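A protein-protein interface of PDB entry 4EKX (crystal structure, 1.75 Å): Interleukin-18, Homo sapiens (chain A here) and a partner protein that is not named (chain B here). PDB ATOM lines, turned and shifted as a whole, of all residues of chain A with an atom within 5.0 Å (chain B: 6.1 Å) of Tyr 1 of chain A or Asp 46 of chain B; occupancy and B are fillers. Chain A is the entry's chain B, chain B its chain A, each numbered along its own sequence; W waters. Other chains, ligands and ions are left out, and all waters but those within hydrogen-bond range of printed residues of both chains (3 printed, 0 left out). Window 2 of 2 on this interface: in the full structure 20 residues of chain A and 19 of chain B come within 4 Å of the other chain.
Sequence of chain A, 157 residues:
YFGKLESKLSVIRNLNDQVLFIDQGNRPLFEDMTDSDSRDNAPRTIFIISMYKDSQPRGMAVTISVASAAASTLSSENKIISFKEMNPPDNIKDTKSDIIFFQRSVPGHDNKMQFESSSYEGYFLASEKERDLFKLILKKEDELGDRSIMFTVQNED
Water W1 lies within hydrogen-bond range of OH of Tyr 1 of chain A (2.8 Å) and OD1 of Asp 46 of chain B (2.9 Å).
Water W2 lies within hydrogen-bond range of the side-chain amino group of Lys 53 of chain A (2.9 Å) and the side-chain carboxylate of Asp 46 of chain B (3.4 Å).
Water W3 lies within hydrogen-bond range of N of Val 45 of chain B (3.0 Å), OE1 of Glu 56 of chain B (3.0 Å) and NZ of Lys 53 of chain A (3.2 Å).
OE1 of Glu 56 of chain B is in salt-bridge range of NZ of Lys 53 of chain A, 2.8 Å away.
The side-chain amino group (NZ) of Lys 53 of chain A lies within salt-bridge range of the side-chain carboxylate (OD2) of Asp 46 of chain B (2.7 Å).
Tyr 1 of chain A touches three residues of chain B.
Printed residues of chain B within 4 Å of Ser 55 of chain A: Asn 42, Thr 44 and Gln 47.
Of the printed residues of chain A, Asn 42 of chain B touches Ser 55 (3.1 Å).
Of chain A, only Tyr 1 (3.5 Å) and Lys 53 (2.7 Å) come within 4 Å of Asp 46 of chain B.
Of the printed residues of chain A, Glu 56 of chain B touches Lys 53 (2.8 Å).
The nearest printed residue of chain A that does not touch Asp 46 of chain B is Gly 3 of chain A (5.5 Å).
Hydrophobic or aromatic side chains of chain A that line the printed part of chain B: Tyr 1.
Of the 8 printed residues of chain B, 5 touch a printed residue of chain A.
Among the printed residues, Asp or Glu carboxylates within 4 Å of a Lys or Arg side-chain nitrogen of the other chain: Lys 53 of chain A with Asp 46 of chain B (2.7 Å) and Lys 53 of chain A with Glu 56 of chain B (2.8 Å).
The backbone carbonyl oxygen (O) of Asp 94 of chain A sits at hydrogen-bond distance from the backbone NH (N) of Tyr 1 of chain A, at 3.0 Å.
OG of Ser 55 of chain A lies within hydrogen-bond range of N of Tyr 1 of chain A.
The side-chain amide oxygen (OD1) of Asn 42 of chain B is in hydrogen-bond range of the side-chain amino group (NZ) of Lys 43 of chain B, at 2.9 Å.
The backbone carbonyl oxygen of Gly 3 of chain A lies within hydrogen-bond range of the backbone NH of Lys 53 of chain A (2.9 Å).
The side-chain amide oxygen (OE1) of Gln 47 of chain B is in hydrogen-bond range of the backbone NH (N) of Thr 44 of chain B, at 2.9 Å.
Among the printed residues, pairs that only touch across the chains: Ser 55 of chain A with Asn 42 of chain B (3.1 Å), Tyr 1 of chain A with Gln 47 of chain B (3.4 Å), Ser 55 of chain A with Gln 47 of chain B (3.4 Å), Tyr 1 of chain A with Asp 46 of chain B (3.5 Å), Tyr 1 of chain A with Thr 44 of chain B (3.6 Å), Lys 53 of chain A with Thr 44 of chain B (3.9 Å) and Ser 55 of chain A with Thr 44 of chain B (3.95 Å).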
ATOM      1  N   TYR A   1     -14.355  11.244 -23.051  1.00  0.00           N
ATOM      2  CA  TYR A   1     -15.370  10.499 -22.315  1.00  0.00           C
ATOM      3  C   TYR A   1     -14.876   9.088 -21.982  1.00  0.00           C
ATOM      4  O   TYR A   1     -14.435   8.375 -22.877  1.00  0.00           O
ATOM      5  CB  TYR A   1     -16.628  10.359 -23.176  1.00  0.00           C
ATOM      6  CG  TYR A   1     -17.743   9.621 -22.479  1.00  0.00           C
ATOM      7  CD1 TYR A   1     -18.623  10.299 -21.641  1.00  0.00           C
ATOM      8  CD2 TYR A   1     -17.914   8.248 -22.645  1.00  0.00           C
ATOM      9  CE1 TYR A   1     -19.646   9.638 -20.995  1.00  0.00           C
ATOM     10  CE2 TYR A   1     -18.948   7.571 -21.999  1.00  0.00           C
ATOM     11  CZ  TYR A   1     -19.809   8.279 -21.171  1.00  0.00           C
ATOM     12  OH  TYR A   1     -20.841   7.633 -20.519  1.00  0.00           O
ATOM     13  N   PHE A   2     -14.967   8.705 -20.705  1.00  0.00           N
ATOM     14  CA  PHE A   2     -14.691   7.336 -20.266  1.00  0.00           C
ATOM     15  C   PHE A   2     -15.971   6.701 -19.726  1.00  0.00           C
ATOM     16  O   PHE A   2     -16.645   7.281 -18.876  1.00  0.00           O
ATOM     17  CB  PHE A   2     -13.656   7.327 -19.136  1.00  0.00           C
ATOM     18  CG  PHE A   2     -12.336   7.922 -19.504  1.00  0.00           C
ATOM     19  CD1 PHE A   2     -11.429   7.204 -20.267  1.00  0.00           C
ATOM     20  CD2 PHE A   2     -11.983   9.193 -19.066  1.00  0.00           C
ATOM     21  CE1 PHE A   2     -10.184   7.749 -20.588  1.00  0.00           C
ATOM     22  CE2 PHE A   2     -10.742   9.740 -19.388  1.00  0.00           C
ATOM     23  CZ  PHE A   2      -9.837   9.002 -20.152  1.00  0.00           C
ATOM     24  N   GLY A   3     -16.287   5.497 -20.193  1.00  0.00           N
ATOM     25  CA  GLY A   3     -17.452   4.774 -19.715  1.00  0.00           C
ATOM     26  C   GLY A   3     -17.031   3.428 -19.148  1.00  0.00           C
ATOM     27  O   GLY A   3     -16.342   2.649 -19.815  1.00  0.00           O
ATOM     28  N   LYS A  53     -14.240   2.210 -21.706  1.00  0.00           N
ATOM     29  CA  LYS A  53     -14.191   2.623 -23.100  1.00  0.00           C
ATOM     30  C   LYS A  53     -13.830   4.113 -23.148  1.00  0.00           C
ATOM     31  O   LYS A  53     -14.072   4.857 -22.191  1.00  0.00           O
ATOM     32  CB  LYS A  53     -15.554   2.386 -23.785  1.00  0.00           C
ATOM     33  CG  LYS A  53     -16.658   3.253 -23.212  1.00  0.00           C
ATOM     34  CD  LYS A  53     -17.925   3.238 -24.073  1.00  0.00           C
ATOM     35  CE  LYS A  53     -18.602   1.902 -24.064  1.00  0.00           C
ATOM     36  NZ  LYS A  53     -19.964   1.971 -24.701  1.00  0.00           N
ATOM     37  N   ASP A  54     -13.247   4.538 -24.264  1.00  0.00           N
ATOM     38  CA  ASP A  54     -12.734   5.893 -24.415  1.00  0.00           C
ATOM     39  C   ASP A  54     -13.210   6.481 -25.753  1.00  0.00           C
ATOM     40  O   ASP A  54     -13.061   5.854 -26.796  1.00  0.00           O
ATOM     41  CB  ASP A  54     -11.193   5.838 -24.348  1.00  0.00           C
ATOM     42  CG  ASP A  54     -10.563   7.192 -24.118  1.00  0.00           C
ATOM     43  OD1 ASP A  54     -11.255   8.219 -24.325  1.00  0.00           O
ATOM     44  OD2 ASP A  54      -9.363   7.229 -23.741  1.00  0.00           O
ATOM     45  N   SER A  55     -13.766   7.691 -25.731  1.00  0.00           N
ATOM     46  CA  SER A  55     -14.179   8.333 -26.974  1.00  0.00           C
ATOM     47  C   SER A  55     -12.952   8.708 -27.798  1.00  0.00           C
ATOM     48  O   SER A  55     -13.057   8.987 -28.994  1.00  0.00           O
ATOM     49  CB  SER A  55     -15.005   9.583 -26.676  1.00  0.00           C
ATOM     50  OG  SER A  55     -14.330  10.418 -25.750  1.00  0.00           O
ATOM     51  N   ASN A  91     -19.118   6.821 -15.290  1.00  0.00           N
ATOM     52  CA  ASN A  91     -18.519   7.525 -16.416  1.00  0.00           C
ATOM     53  C   ASN A  91     -17.738   8.752 -15.972  1.00  0.00           C
ATOM     54  O   ASN A  91     -17.919   9.249 -14.865  1.00  0.00           O
ATOM     55  CB  ASN A  91     -19.564   7.893 -17.483  1.00  0.00           C
ATOM     56  CG  ASN A  91     -20.593   8.887 -16.982  1.00  0.00           C
ATOM     57  OD1 ASN A  91     -20.358  10.097 -16.983  1.00  0.00           O
ATOM     58  ND2 ASN A  91     -21.748   8.383 -16.561  1.00  0.00           N
ATOM     59  N   ILE A  92     -16.862   9.219 -16.848  1.00  0.00           N
ATOM     60  CA  ILE A  92     -16.114  10.434 -16.614  1.00  0.00           C
ATOM     61  C   ILE A  92     -16.229  11.284 -17.871  1.00  0.00           C
ATOM     62  O   ILE A  92     -15.803  10.872 -18.946  1.00  0.00           O
ATOM     63  CB  ILE A  92     -14.644  10.127 -16.300  1.00  0.00           C
ATOM     64  CG1 ILE A  92     -14.547   9.411 -14.951  1.00  0.00           C
ATOM     65  CG2 ILE A  92     -13.831  11.410 -16.299  1.00  0.00           C
ATOM     66  CD1 ILE A  92     -13.250   8.638 -14.752  1.00  0.00           C
ATOM     67  N   LYS A  93     -16.816  12.468 -17.739  1.00  0.00           N
ATOM     68  CA  LYS A  93     -17.097  13.288 -18.915  1.00  0.00           C
ATOM     69  C   LYS A  93     -15.909  14.234 -19.077  1.00  0.00           C
ATOM     70  O   LYS A  93     -15.997  15.427 -18.781  1.00  0.00           O
ATOM     71  CB  LYS A  93     -18.431  14.024 -18.758  1.00  0.00           C
ATOM     72  CG  LYS A  93     -19.606  13.070 -18.623  1.00  0.00           C
ATOM     73  CD  LYS A  93     -20.909  13.830 -18.417  1.00  0.00           C
ATOM     74  CE  LYS A  93     -22.128  12.950 -18.660  1.00  0.00           C
ATOM     75  NZ  LYS A  93     -22.399  12.002 -17.541  1.00  0.00           N
ATOM     76  N   ASP A  94     -14.793  13.670 -19.532  1.00  0.00           N
ATOM     77  CA  ASP A  94     -13.561  14.419 -19.752  1.00  0.00           C
ATOM     78  C   ASP A  94     -12.635  13.461 -20.493  1.00  0.00           C
ATOM     79  O   ASP A  94     -12.924  12.252 -20.567  1.00  0.00           O
ATOM     80  CB  ASP A  94     -12.916  14.907 -18.441  1.00  0.00           C
ATOM     81  CG  ASP A  94     -11.975  16.086 -18.644  1.00  0.00           C
ATOM     82  OD1 ASP A  94     -11.663  16.422 -19.807  1.00  0.00           O
ATOM     83  OD2 ASP A  94     -11.545  16.686 -17.633  1.00  0.00           O
ATOM     84  N   THR A  95     -11.530  13.966 -21.041  1.00  0.00           N
ATOM     85  CA  THR A  95     -10.590  13.061 -21.713  1.00  0.00           C
ATOM     86  C   THR A  95      -9.378  12.710 -20.855  1.00  0.00           C
ATOM     87  O   THR A  95      -8.460  12.032 -21.315  1.00  0.00           O
ATOM     88  CB  THR A  95     -10.112  13.639 -23.044  1.00  0.00           C
ATOM     89  OG1 THR A  95      -9.508  14.912 -22.803  1.00  0.00           O
ATOM     90  CG2 THR A  95     -11.288  13.804 -24.000  1.00  0.00           C
ATOM     91  N   ASN B  42     -15.941  11.032 -32.631  1.00  0.00           N
ATOM     92  CA  ASN B  42     -15.591  10.869 -31.216  1.00  0.00           C
ATOM     93  C   ASN B  42     -16.721  10.608 -30.225  1.00  0.00           C
ATOM     94  O   ASN B  42     -16.544  10.800 -29.018  1.00  0.00           O
ATOM     95  CB  ASN B  42     -14.769  12.078 -30.756  1.00  0.00           C
ATOM     96  CG  ASN B  42     -15.524  13.389 -30.908  1.00  0.00           C
ATOM     97  OD1 ASN B  42     -16.742  13.402 -31.126  1.00  0.00           O
ATOM     98  ND2 ASN B  42     -14.808  14.501 -30.777  1.00  0.00           N
ATOM     99  N   LYS B  43     -17.883  10.192 -30.718  1.00  0.00           N
ATOM    100  CA  LYS B  43     -18.983   9.869 -29.819  1.00  0.00           C
ATOM    101  C   LYS B  43     -19.161   8.365 -29.597  1.00  0.00           C
ATOM    102  O   LYS B  43     -19.442   7.627 -30.532  1.00  0.00           O
ATOM    103  CB  LYS B  43     -20.279  10.485 -30.374  1.00  0.00           C
ATOM    104  CG  LYS B  43     -20.214  11.998 -30.548  1.00  0.00           C
ATOM    105  CD  LYS B  43     -20.125  12.699 -29.208  1.00  0.00           C
ATOM    106  CE  LYS B  43     -20.214  14.217 -29.358  1.00  0.00           C
ATOM    107  NZ  LYS B  43     -19.249  14.753 -30.366  1.00  0.00           N
ATOM    108  N   THR B  44     -18.976   7.911 -28.360  1.00  0.00           N
ATOM    109  CA  THR B  44     -19.460   6.591 -27.999  1.00  0.00           C
ATOM    110  C   THR B  44     -20.980   6.681 -27.988  1.00  0.00           C
ATOM    111  O   THR B  44     -21.543   7.782 -27.904  1.00  0.00           O
ATOM    112  CB  THR B  44     -18.992   6.137 -26.612  1.00  0.00           C
ATOM    113  OG1 THR B  44     -19.590   6.959 -25.603  1.00  0.00           O
ATOM    114  CG2 THR B  44     -17.470   6.195 -26.515  1.00  0.00           C
ATOM    115  N   VAL B  45     -21.634   5.526 -28.048  1.00  0.00           N
ATOM    116  CA  VAL B  45     -23.095   5.469 -28.079  1.00  0.00           C
ATOM    117  C   VAL B  45     -23.681   6.094 -26.810  1.00  0.00           C
ATOM    118  O   VAL B  45     -24.732   6.730 -26.847  1.00  0.00           O
ATOM    119  CB  VAL B  45     -23.583   4.010 -28.276  1.00  0.00           C
ATOM    120  CG1 VAL B  45     -25.113   3.927 -28.248  1.00  0.00           C
ATOM    121  CG2 VAL B  45     -23.061   3.470 -29.603  1.00  0.00           C
ATOM    122  N   ASP B  46     -22.974   5.935 -25.696  1.00  0.00           N
ATOM    123  CA  ASP B  46     -23.380   6.503 -24.410  1.00  0.00           C
ATOM    124  C   ASP B  46     -23.555   8.017 -24.480  1.00  0.00           C
ATOM    125  O   ASP B  46     -24.333   8.602 -23.721  1.00  0.00           O
ATOM    126  CB  ASP B  46     -22.326   6.184 -23.339  1.00  0.00           C
ATOM    127  CG  ASP B  46     -21.988   4.699 -23.278  1.00  0.00           C
ATOM    128  OD1 ASP B  46     -22.245   4.074 -22.229  1.00  0.00           O
ATOM    129  OD2 ASP B  46     -21.485   4.157 -24.287  1.00  0.00           O
ATOM    130  N   GLN B  47     -22.829   8.652 -25.391  1.00  0.00           N
ATOM    131  CA  GLN B  47     -22.835  10.118 -25.474  1.00  0.00           C
ATOM    132  C   GLN B  47     -23.931  10.704 -26.364  1.00  0.00           C
ATOM    133  O   GLN B  47     -24.195  11.913 -26.331  1.00  0.00           O
ATOM    134  CB  GLN B  47     -21.472  10.609 -25.948  1.00  0.00           C
ATOM    135  CG  GLN B  47     -20.352  10.318 -24.969  1.00  0.00           C
ATOM    136  CD  GLN B  47     -19.000  10.550 -25.597  1.00  0.00           C
ATOM    137  OE1 GLN B  47     -18.384   9.617 -26.116  1.00  0.00           O
ATOM    138  NE2 GLN B  47     -18.542  11.804 -25.581  1.00  0.00           N
ATOM    139  N   LEU B  48     -24.574   9.852 -27.152  1.00  0.00           N
ATOM    140  CA  LEU B  48     -25.614  10.313 -28.077  1.00  0.00           C
ATOM    141  C   LEU B  48     -26.891  10.756 -27.367  1.00  0.00           C
ATOM    142  O   LEU B  48     -27.240  10.240 -26.305  1.00  0.00           O
ATOM    143  CB  LEU B  48     -25.944   9.212 -29.087  1.00  0.00           C
ATOM    144  CG  LEU B  48     -24.739   8.728 -29.896  1.00  0.00           C
ATOM    145  CD1 LEU B  48     -25.129   7.557 -30.781  1.00  0.00           C
ATOM    146  CD2 LEU B  48     -24.202   9.886 -30.724  1.00  0.00           C
ATOM    147  N   GLU B  56     -26.212   0.122 -28.436  1.00  0.00           N
ATOM    148  CA  GLU B  56     -25.075  -0.785 -28.407  1.00  0.00           C
ATOM    149  C   GLU B  56     -25.313  -1.929 -27.436  1.00  0.00           C
ATOM    150  O   GLU B  56     -25.846  -1.736 -26.342  1.00  0.00           O
ATOM    151  CB  GLU B  56     -23.797  -0.037 -28.029  1.00  0.00           C
ATOM    152  CG  GLU B  56     -22.554  -0.904 -28.042  1.00  0.00           C
ATOM    153  CD  GLU B  56     -21.325  -0.105 -27.693  1.00  0.00           C
ATOM    154  OE1 GLU B  56     -21.331   0.524 -26.616  1.00  0.00           O
ATOM    155  OE2 GLU B  56     -20.367  -0.094 -28.494  1.00  0.00           O
HETATM  156  O   HOH W   1     -20.895   4.936 -19.857  1.00  0.00           O
HETATM  157  O   HOH W   2     -21.135   0.908 -22.302  1.00  0.00           O
HETATM  158  O   HOH W   3     -19.956   3.004 -27.732  1.00  0.00           O
